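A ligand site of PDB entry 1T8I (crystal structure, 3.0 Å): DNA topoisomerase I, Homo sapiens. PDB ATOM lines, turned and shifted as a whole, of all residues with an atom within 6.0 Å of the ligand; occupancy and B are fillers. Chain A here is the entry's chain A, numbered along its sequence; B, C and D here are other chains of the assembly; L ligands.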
ATOM      1  N   ASN A 179      21.350  -8.407 -18.846  1.00  0.00           N
ATOM      2  CA  ASN A 179      22.743  -7.949 -18.940  1.00  0.00           C
ATOM      3  C   ASN A 179      23.666  -9.176 -18.947  1.00  0.00           C
ATOM      4  O   ASN A 179      24.517  -9.341 -18.045  1.00  0.00           O
ATOM      5  CB  ASN A 179      23.079  -7.125 -17.684  1.00  0.00           C
ATOM      6  CG  ASN A 179      22.660  -5.642 -17.767  1.00  0.00           C
ATOM      7  OD1 ASN A 179      23.442  -4.758 -17.362  1.00  0.00           O
ATOM      8  ND2 ASN A 179      21.433  -5.362 -18.197  1.00  0.00           N
ATOM      9  N   GLU A 183      30.389  -7.665 -16.229  1.00  0.00           N
ATOM     10  CA  GLU A 183      31.073  -6.384 -16.109  1.00  0.00           C
ATOM     11  C   GLU A 183      32.594  -6.494 -16.003  1.00  0.00           C
ATOM     12  O   GLU A 183      33.098  -7.320 -15.282  1.00  0.00           O
ATOM     13  CB  GLU A 183      30.465  -5.643 -14.897  1.00  0.00           C
ATOM     14  CG  GLU A 183      30.298  -4.091 -15.042  1.00  0.00           C
ATOM     15  CD  GLU A 183      29.414  -3.646 -16.258  1.00  0.00           C
ATOM     16  OE1 GLU A 183      29.992  -3.370 -17.348  1.00  0.00           O
ATOM     17  OE2 GLU A 183      28.161  -3.542 -16.098  1.00  0.00           O
ATOM     18  N   ARG A 191      28.898   6.159  -6.065  1.00  0.00           N
ATOM     19  CA  ARG A 191      28.292   7.485  -6.077  1.00  0.00           C
ATOM     20  C   ARG A 191      28.489   8.127  -4.725  1.00  0.00           C
ATOM     21  O   ARG A 191      28.630   7.446  -3.710  1.00  0.00           O
ATOM     22  CB  ARG A 191      26.813   7.436  -6.445  1.00  0.00           C
ATOM     23  CG  ARG A 191      26.316   6.150  -7.134  1.00  0.00           C
ATOM     24  CD  ARG A 191      24.926   6.357  -7.696  1.00  0.00           C
ATOM     25  NE  ARG A 191      24.337   5.148  -8.242  1.00  0.00           N
ATOM     26  CZ  ARG A 191      24.562   4.662  -9.479  1.00  0.00           C
ATOM     27  NH1 ARG A 191      25.385   5.300 -10.347  1.00  0.00           N
ATOM     28  NH2 ARG A 191      23.910   3.557  -9.877  1.00  0.00           N
ATOM     29  N   LYS A 252      25.970 -10.251  -7.206  1.00  0.00           N
ATOM     30  CA  LYS A 252      25.474  -9.733  -8.485  1.00  0.00           C
ATOM     31  C   LYS A 252      24.731 -10.856  -9.187  1.00  0.00           C
ATOM     32  O   LYS A 252      24.946 -12.025  -8.843  1.00  0.00           O
ATOM     33  CB  LYS A 252      26.609  -9.235  -9.369  1.00  0.00           C
ATOM     34  CG  LYS A 252      27.402  -8.052  -8.803  1.00  0.00           C
ATOM     35  CD  LYS A 252      26.580  -6.812  -8.611  1.00  0.00           C
ATOM     36  CE  LYS A 252      27.422  -5.610  -8.250  1.00  0.00           C
ATOM     37  NZ  LYS A 252      26.545  -4.382  -8.149  1.00  0.00           N
ATOM     38  N   ARG A 315      11.933   7.657   1.758  1.00  0.00           N
ATOM     39  CA  ARG A 315      12.156   6.231   1.655  1.00  0.00           C
ATOM     40  C   ARG A 315      12.214   5.704   3.100  1.00  0.00           C
ATOM     41  O   ARG A 315      12.472   6.468   4.040  1.00  0.00           O
ATOM     42  CB  ARG A 315      13.496   5.998   0.963  1.00  0.00           C
ATOM     43  CG  ARG A 315      13.523   6.374  -0.494  1.00  0.00           C
ATOM     44  CD  ARG A 315      14.904   6.185  -1.065  1.00  0.00           C
ATOM     45  NE  ARG A 315      14.909   6.121  -2.523  1.00  0.00           N
ATOM     46  CZ  ARG A 315      14.858   7.169  -3.344  1.00  0.00           C
ATOM     47  NH1 ARG A 315      14.777   8.396  -2.862  1.00  0.00           N
ATOM     48  NH2 ARG A 315      15.008   6.994  -4.649  1.00  0.00           N
ATOM     49  N   LYS A 359      19.153   8.797  -1.174  1.00  0.00           N
ATOM     50  CA  LYS A 359      19.736   7.687  -1.929  1.00  0.00           C
ATOM     51  C   LYS A 359      20.592   8.315  -3.008  1.00  0.00           C
ATOM     52  O   LYS A 359      20.229   9.365  -3.546  1.00  0.00           O
ATOM     53  CB  LYS A 359      18.670   6.796  -2.574  1.00  0.00           C
ATOM     54  CG  LYS A 359      19.222   5.530  -3.271  1.00  0.00           C
ATOM     55  CD  LYS A 359      18.161   4.688  -4.003  1.00  0.00           C
ATOM     56  CE  LYS A 359      18.818   3.752  -5.035  1.00  0.00           C
ATOM     57  NZ  LYS A 359      18.067   2.477  -5.247  1.00  0.00           N
ATOM     58  N   ASP A 360      21.752   7.690  -3.278  1.00  0.00           N
ATOM     59  CA  ASP A 360      22.726   8.161  -4.290  1.00  0.00           C
ATOM     60  C   ASP A 360      23.303   9.548  -3.966  1.00  0.00           C
ATOM     61  O   ASP A 360      23.574  10.333  -4.873  1.00  0.00           O
ATOM     62  CB  ASP A 360      22.082   8.183  -5.690  1.00  0.00           C
ATOM     63  CG  ASP A 360      21.411   6.867  -6.048  1.00  0.00           C
ATOM     64  OD1 ASP A 360      22.015   5.806  -5.745  1.00  0.00           O
ATOM     65  OD2 ASP A 360      20.288   6.887  -6.599  1.00  0.00           O
ATOM     66  N   HIS A 459      13.615  13.130  -7.794  1.00  0.00           N
ATOM     67  CA  HIS A 459      14.531  12.583  -8.807  1.00  0.00           C
ATOM     68  C   HIS A 459      15.218  13.731  -9.504  1.00  0.00           C
ATOM     69  O   HIS A 459      14.839  14.131 -10.613  1.00  0.00           O
ATOM     70  CB  HIS A 459      13.787  11.688  -9.805  1.00  0.00           C
ATOM     71  CG  HIS A 459      13.267  10.429  -9.208  1.00  0.00           C
ATOM     72  ND1 HIS A 459      12.132   9.812  -9.688  1.00  0.00           N
ATOM     73  CD2 HIS A 459      13.681   9.704  -8.146  1.00  0.00           C
ATOM     74  CE1 HIS A 459      11.866   8.769  -8.929  1.00  0.00           C
ATOM     75  NE2 HIS A 459      12.782   8.668  -7.986  1.00  0.00           N
ATOM     76  N   THR A 545      13.367   7.454 -13.735  1.00  0.00           N
ATOM     77  CA  THR A 545      13.112   6.580 -12.590  1.00  0.00           C
ATOM     78  C   THR A 545      11.623   6.443 -12.270  1.00  0.00           C
ATOM     79  O   THR A 545      11.163   5.373 -11.919  1.00  0.00           O
ATOM     80  CB  THR A 545      14.057   6.938 -11.369  1.00  0.00           C
ATOM     81  OG1 THR A 545      15.433   6.750 -11.744  1.00  0.00           O
ATOM     82  CG2 THR A 545      13.777   6.019 -10.159  1.00  0.00           C
ATOM     83  N   ASN A 549      10.119   2.982 -13.207  1.00  0.00           N
ATOM     84  CA  ASN A 549       9.909   2.386 -11.910  1.00  0.00           C
ATOM     85  C   ASN A 549       8.694   2.699 -11.027  1.00  0.00           C
ATOM     86  O   ASN A 549       8.274   1.808 -10.282  1.00  0.00           O
ATOM     87  CB  ASN A 549      11.202   2.508 -11.106  1.00  0.00           C
ATOM     88  CG  ASN A 549      12.327   1.709 -11.709  1.00  0.00           C
ATOM     89  OD1 ASN A 549      13.313   2.277 -12.225  1.00  0.00           O
ATOM     90  ND2 ASN A 549      12.196   0.380 -11.650  1.00  0.00           N
ATOM     91  N   PTR A 550       8.076   3.870 -11.151  1.00  0.00           N
ATOM     92  CA  PTR A 550       6.962   4.215 -10.243  1.00  0.00           C
ATOM     93  C   PTR A 550       5.514   4.353 -10.641  1.00  0.00           C
ATOM     94  O   PTR A 550       4.624   4.198  -9.800  1.00  0.00           O
ATOM     95  CB  PTR A 550       7.306   5.469  -9.478  1.00  0.00           C
ATOM     96  CG  PTR A 550       8.384   5.241  -8.494  1.00  0.00           C
ATOM     97  CD1 PTR A 550       9.591   5.948  -8.583  1.00  0.00           C
ATOM     98  CD2 PTR A 550       8.216   4.317  -7.465  1.00  0.00           C
ATOM     99  CE1 PTR A 550      10.628   5.718  -7.650  1.00  0.00           C
ATOM    100  CE2 PTR A 550       9.239   4.080  -6.548  1.00  0.00           C
ATOM    101  CZ  PTR A 550      10.438   4.776  -6.632  1.00  0.00           C
ATOM    102  OH  PTR A 550      11.379   4.446  -5.704  1.00  0.00           O
ATOM    103  P   PTR A 550      12.910   4.870  -5.775  1.00  0.00           P
ATOM    104  O1P PTR A 550      13.173   6.331  -5.970  1.00  0.00           O
ATOM    105  O2P PTR A 550      13.627   4.126  -4.683  1.00  0.00           O
ATOM    106  O3P PTR A 550      13.518   4.195  -7.087  1.00  0.00           O
ATOM    107  P    DT B  10      10.469  -0.615  -7.413  1.00  0.00           P
ATOM    108  OP1  DT B  10       9.363  -0.019  -6.614  1.00  0.00           O
ATOM    109  OP2  DT B  10      10.247  -0.969  -8.866  1.00  0.00           O
ATOM    110  O5'  DT B  10      11.756   0.362  -7.353  1.00  0.00           O
ATOM    111  C5'  DT B  10      12.267   0.863  -6.099  1.00  0.00           C
ATOM    112  C4'  DT B  10      13.360   1.893  -6.331  1.00  0.00           C
ATOM    113  O4'  DT B  10      14.673   1.338  -6.632  1.00  0.00           O
ATOM    114  C3'  DT B  10      13.046   2.900  -7.434  1.00  0.00           C
ATOM    115  C2'  DT B  10      14.017   2.538  -8.545  1.00  0.00           C
ATOM    116  C1'  DT B  10      15.221   1.987  -7.787  1.00  0.00           C
ATOM    117  N1   DT B  10      16.079   1.016  -8.515  1.00  0.00           N
ATOM    118  C2   DT B  10      17.461   1.196  -8.481  1.00  0.00           C
ATOM    119  O2   DT B  10      18.006   2.187  -7.994  1.00  0.00           O
ATOM    120  N3   DT B  10      18.193   0.194  -9.050  1.00  0.00           N
ATOM    121  C4   DT B  10      17.725  -0.920  -9.684  1.00  0.00           C
ATOM    122  O4   DT B  10      18.511  -1.745 -10.125  1.00  0.00           O
ATOM    123  C5   DT B  10      16.284  -1.026  -9.772  1.00  0.00           C
ATOM    124  C7   DT B  10      15.696  -2.184 -10.507  1.00  0.00           C
ATOM    125  C6   DT B  10      15.535  -0.068  -9.183  1.00  0.00           C
ATOM    126  S5' TGP C   1      15.822   5.005 -17.256  1.00  0.00           S
ATOM    127  N9  TGP C   1      19.542   3.514 -14.801  1.00  0.00           N
ATOM    128  C4  TGP C   1      20.888   3.277 -14.721  1.00  0.00           C
ATOM    129  N3  TGP C   1      21.818   4.143 -14.307  1.00  0.00           N
ATOM    130  C2  TGP C   1      23.017   3.609 -14.313  1.00  0.00           C
ATOM    131  N2  TGP C   1      24.073   4.302 -13.875  1.00  0.00           N
ATOM    132  N1  TGP C   1      23.286   2.348 -14.734  1.00  0.00           N
ATOM    133  C6  TGP C   1      22.340   1.439 -15.186  1.00  0.00           C
ATOM    134  O6  TGP C   1      22.692   0.306 -15.564  1.00  0.00           O
ATOM    135  C5  TGP C   1      21.055   1.974 -15.149  1.00  0.00           C
ATOM    136  N7  TGP C   1      19.833   1.404 -15.479  1.00  0.00           N
ATOM    137  C8  TGP C   1      18.967   2.352 -15.261  1.00  0.00           C
ATOM    138  C2' TGP C   1      18.741   5.737 -15.578  1.00  0.00           C
ATOM    139  C5' TGP C   1      15.518   4.855 -15.396  1.00  0.00           C
ATOM    140  C4' TGP C   1      16.628   5.460 -14.555  1.00  0.00           C
ATOM    141  O4' TGP C   1      17.533   4.429 -14.079  1.00  0.00           O
ATOM    142  C1' TGP C   1      18.857   4.755 -14.450  1.00  0.00           C
ATOM    143  C3' TGP C   1      17.536   6.554 -15.143  1.00  0.00           C
ATOM    144  O3' TGP C   1      17.976   7.467 -14.118  1.00  0.00           O
ATOM    145  P    DG C   2      17.164   8.832 -13.818  1.00  0.00           P
ATOM    146  OP1  DG C   2      16.716   8.793 -12.411  1.00  0.00           O
ATOM    147  OP2  DG C   2      16.155   9.122 -14.900  1.00  0.00           O
ATOM    148  O5'  DG C   2      18.283   9.953 -13.870  1.00  0.00           O
ATOM    149  C5'  DG C   2      19.249  10.049 -12.845  1.00  0.00           C
ATOM    150  C4'  DG C   2      20.619  10.157 -13.477  1.00  0.00           C
ATOM    151  O4'  DG C   2      20.840   8.914 -14.181  1.00  0.00           O
ATOM    152  C3'  DG C   2      20.727  11.262 -14.533  1.00  0.00           C
ATOM    153  O3'  DG C   2      21.938  12.032 -14.435  1.00  0.00           O
ATOM    154  C2'  DG C   2      20.699  10.492 -15.857  1.00  0.00           C
ATOM    155  C1'  DG C   2      21.410   9.221 -15.438  1.00  0.00           C
ATOM    156  N9   DG C   2      21.307   8.056 -16.300  1.00  0.00           N
ATOM    157  C8   DG C   2      20.231   7.638 -17.042  1.00  0.00           C
ATOM    158  N7   DG C   2      20.455   6.502 -17.649  1.00  0.00           N
ATOM    159  C5   DG C   2      21.745   6.159 -17.297  1.00  0.00           C
ATOM    160  C6   DG C   2      22.515   5.053 -17.647  1.00  0.00           C
ATOM    161  O6   DG C   2      22.181   4.076 -18.298  1.00  0.00           O
ATOM    162  N1   DG C   2      23.806   5.125 -17.137  1.00  0.00           N
ATOM    163  C2   DG C   2      24.274   6.153 -16.368  1.00  0.00           C
ATOM    164  N2   DG C   2      25.563   6.071 -16.017  1.00  0.00           N
ATOM    165  N3   DG C   2      23.549   7.188 -15.999  1.00  0.00           N
ATOM    166  C4   DG C   2      22.300   7.126 -16.500  1.00  0.00           C
ATOM    167  P    DC D  12      33.171   1.756 -16.614  1.00  0.00           P
ATOM    168  OP1  DC D  12      34.213   2.805 -16.296  1.00  0.00           O
ATOM    169  OP2  DC D  12      33.563   0.294 -16.509  1.00  0.00           O
ATOM    170  O5'  DC D  12      31.934   2.096 -15.647  1.00  0.00           O
ATOM    171  C5'  DC D  12      32.138   2.196 -14.248  1.00  0.00           C
ATOM    172  C4'  DC D  12      30.850   2.503 -13.534  1.00  0.00           C
ATOM    173  O4'  DC D  12      29.669   2.326 -14.363  1.00  0.00           O
ATOM    174  C3'  DC D  12      30.690   1.533 -12.369  1.00  0.00           C
ATOM    175  O3'  DC D  12      30.347   2.190 -11.167  1.00  0.00           O
ATOM    176  C2'  DC D  12      29.545   0.626 -12.785  1.00  0.00           C
ATOM    177  C1'  DC D  12      28.725   1.572 -13.640  1.00  0.00           C
ATOM    178  N1   DC D  12      27.799   0.909 -14.561  1.00  0.00           N
ATOM    179  C2   DC D  12      26.581   1.504 -14.774  1.00  0.00           C
ATOM    180  O2   DC D  12      26.400   2.666 -14.370  1.00  0.00           O
ATOM    181  N3   DC D  12      25.609   0.818 -15.411  1.00  0.00           N
ATOM    182  C4   DC D  12      25.845  -0.415 -15.865  1.00  0.00           C
ATOM    183  N4   DC D  12      24.814  -1.090 -16.406  1.00  0.00           N
ATOM    184  C5   DC D  12      27.145  -0.998 -15.778  1.00  0.00           C
ATOM    185  C6   DC D  12      28.089  -0.292 -15.143  1.00  0.00           C
ATOM    186  P    DA D  13      30.996   1.670  -9.811  1.00  0.00           P
ATOM    187  OP1  DA D  13      32.102   2.617  -9.432  1.00  0.00           O
ATOM    188  OP2  DA D  13      31.261   0.201  -9.983  1.00  0.00           O
ATOM    189  O5'  DA D  13      29.818   1.809  -8.783  1.00  0.00           O
ATOM    190  C5'  DA D  13      28.623   1.142  -9.017  1.00  0.00           C
ATOM    191  C4'  DA D  13      27.560   1.860  -8.249  1.00  0.00           C
ATOM    192  O4'  DA D  13      26.279   1.570  -8.792  1.00  0.00           O
ATOM    193  C3'  DA D  13      27.502   1.588  -6.757  1.00  0.00           C
ATOM    194  O3'  DA D  13      27.355   2.868  -6.121  1.00  0.00           O
ATOM    195  C2'  DA D  13      26.265   0.719  -6.625  1.00  0.00           C
ATOM    196  C1'  DA D  13      25.381   1.206  -7.771  1.00  0.00           C
ATOM    197  N9   DA D  13      24.515   0.224  -8.399  1.00  0.00           N
ATOM    198  C8   DA D  13      24.989  -0.873  -9.015  1.00  0.00           C
ATOM    199  N7   DA D  13      24.069  -1.613  -9.564  1.00  0.00           N
ATOM    200  C5   DA D  13      22.894  -0.972  -9.263  1.00  0.00           C
ATOM    201  C6   DA D  13      21.569  -1.298  -9.528  1.00  0.00           C
ATOM    202  N6   DA D  13      21.227  -2.426 -10.174  1.00  0.00           N
ATOM    203  N1   DA D  13      20.606  -0.466  -9.105  1.00  0.00           N
ATOM    204  C2   DA D  13      20.980   0.633  -8.427  1.00  0.00           C
ATOM    205  N3   DA D  13      22.238   1.051  -8.090  1.00  0.00           N
ATOM    206  C4   DA D  13      23.143   0.177  -8.552  1.00  0.00           C
HETATM  207  O1  LIG L   1      17.119   0.754 -12.476  1.00  0.00           O
HETATM  208  C1  LIG L   1      18.155   1.496 -12.023  1.00  0.00           C
HETATM  209  C2  LIG L   1      17.942   2.694 -11.426  1.00  0.00           C
HETATM  210  C3  LIG L   1      16.516   3.134 -11.314  1.00  0.00           C
HETATM  211  O2  LIG L   1      16.341   3.801 -10.027  1.00  0.00           O
HETATM  212  C4  LIG L   1      17.322   4.648  -9.471  1.00  0.00           C
HETATM  213  O3  LIG L   1      17.103   5.208  -8.306  1.00  0.00           O
HETATM  214  C5  LIG L   1      18.982   3.554 -10.894  1.00  0.00           C
HETATM  215  C6  LIG L   1      20.291   3.005 -11.064  1.00  0.00           C
HETATM  216  C7  LIG L   1      18.617   4.884 -10.207  1.00  0.00           C
HETATM  217  O4  LIG L   1      19.513   5.218  -9.280  1.00  0.00           O
HETATM  218  C8  LIG L   1      18.442   6.030 -11.232  1.00  0.00           C
HETATM  219  C9  LIG L   1      19.473   7.210 -11.070  1.00  0.00           C
HETATM  220  N1  LIG L   1      19.446   1.033 -12.157  1.00  0.00           N
HETATM  221  C10 LIG L   1      19.819  -0.238 -12.763  1.00  0.00           C
HETATM  222  C11 LIG L   1      21.303  -0.219 -12.597  1.00  0.00           C
HETATM  223  C12 LIG L   1      22.282  -1.077 -12.907  1.00  0.00           C
HETATM  224  C13 LIG L   1      23.619  -0.784 -12.613  1.00  0.00           C
HETATM  225  C14 LIG L   1      23.917   0.470 -11.943  1.00  0.00           C
HETATM  226  N2  LIG L   1      22.892   1.439 -11.583  1.00  0.00           N
HETATM  227  C15 LIG L   1      21.650   1.050 -11.915  1.00  0.00           C
HETATM  228  C16 LIG L   1      20.481   1.753 -11.694  1.00  0.00           C
HETATM  229  C17 LIG L   1      24.655  -1.664 -12.944  1.00  0.00           C
HETATM  230  C18 LIG L   1      25.958  -1.338 -12.634  1.00  0.00           C
HETATM  231  C19 LIG L   1      26.255  -0.109 -11.979  1.00  0.00           C
HETATM  232  C20 LIG L   1      25.207   0.826 -11.628  1.00  0.00           C
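O2 of DT 10 of chain B lies close to an oxygen (O2) of the ligand, 3.1 Å away. A nitrogen (N2) of the ligand lies close to N1 of TGP 1 of chain C. Lys 359 touches the ligand (CE to O3, 3.97 Å). Thr 545 touches the ligand. Asn 549 touches the ligand (OD1 to C3, 3.4 Å). PTR 550 touches the ligand (O3P to O3, 3.9 Å). DG 2 of chain C touches the ligand (C5' to C9, 3.4 Å). N1 of DC 12 of chain D touches C19 of the ligand, at 3.2 Å. O4' of DA 13 of chain D touches C20 of the ligand (3.1 Å). 11 residues have an atom within 4 Å of the ligand: Arg 191, Lys 359, Asp 360, Thr 545, Asn 549, PTR 550, DT 10 of chain B, TGP 1 of chain C, DG 2 of chain C, DC 12 of chain D and DA 13 of chain D.
O4 of the ligand is in hydrogen-bond range of OD2 of Asp 360 (3.3 Å). N2 of the ligand lies within hydrogen-bond range of NH2 of Arg 191.
O2 of DT 10 of chain B sits at hydrogen-bond distance from the side-chain amino group of Lys 359, at 2.8 Å. O6 of TGP 1 of chain C sits close to N4 of DC 12 of chain D, 2.7 Å away. The side-chain hydroxyl (OG1) of Thr 545 lies within hydrogen-bond range of OP1 of DG 2 of chain C (2.5 Å). NH2 of Arg 191 lies within hydrogen-bond range of O4' of DA 13 of chain D (3.3 Å). O2P of PTR 550 lies within salt-bridge range of NH2 of Arg 315, at 3.2 Å. C3' of DT 10 of chain B is covalently linked to O3P of PTR 550, at 1.4 Å. The guanidinium group (NE) of Arg 191 is in salt-bridge range of the side-chain carboxylate (OD1) of Asp 360 (3.5 Å). N3 of DT 10 of chain B lies close to N1 of DA 13 of chain D, 2.5 Å away.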
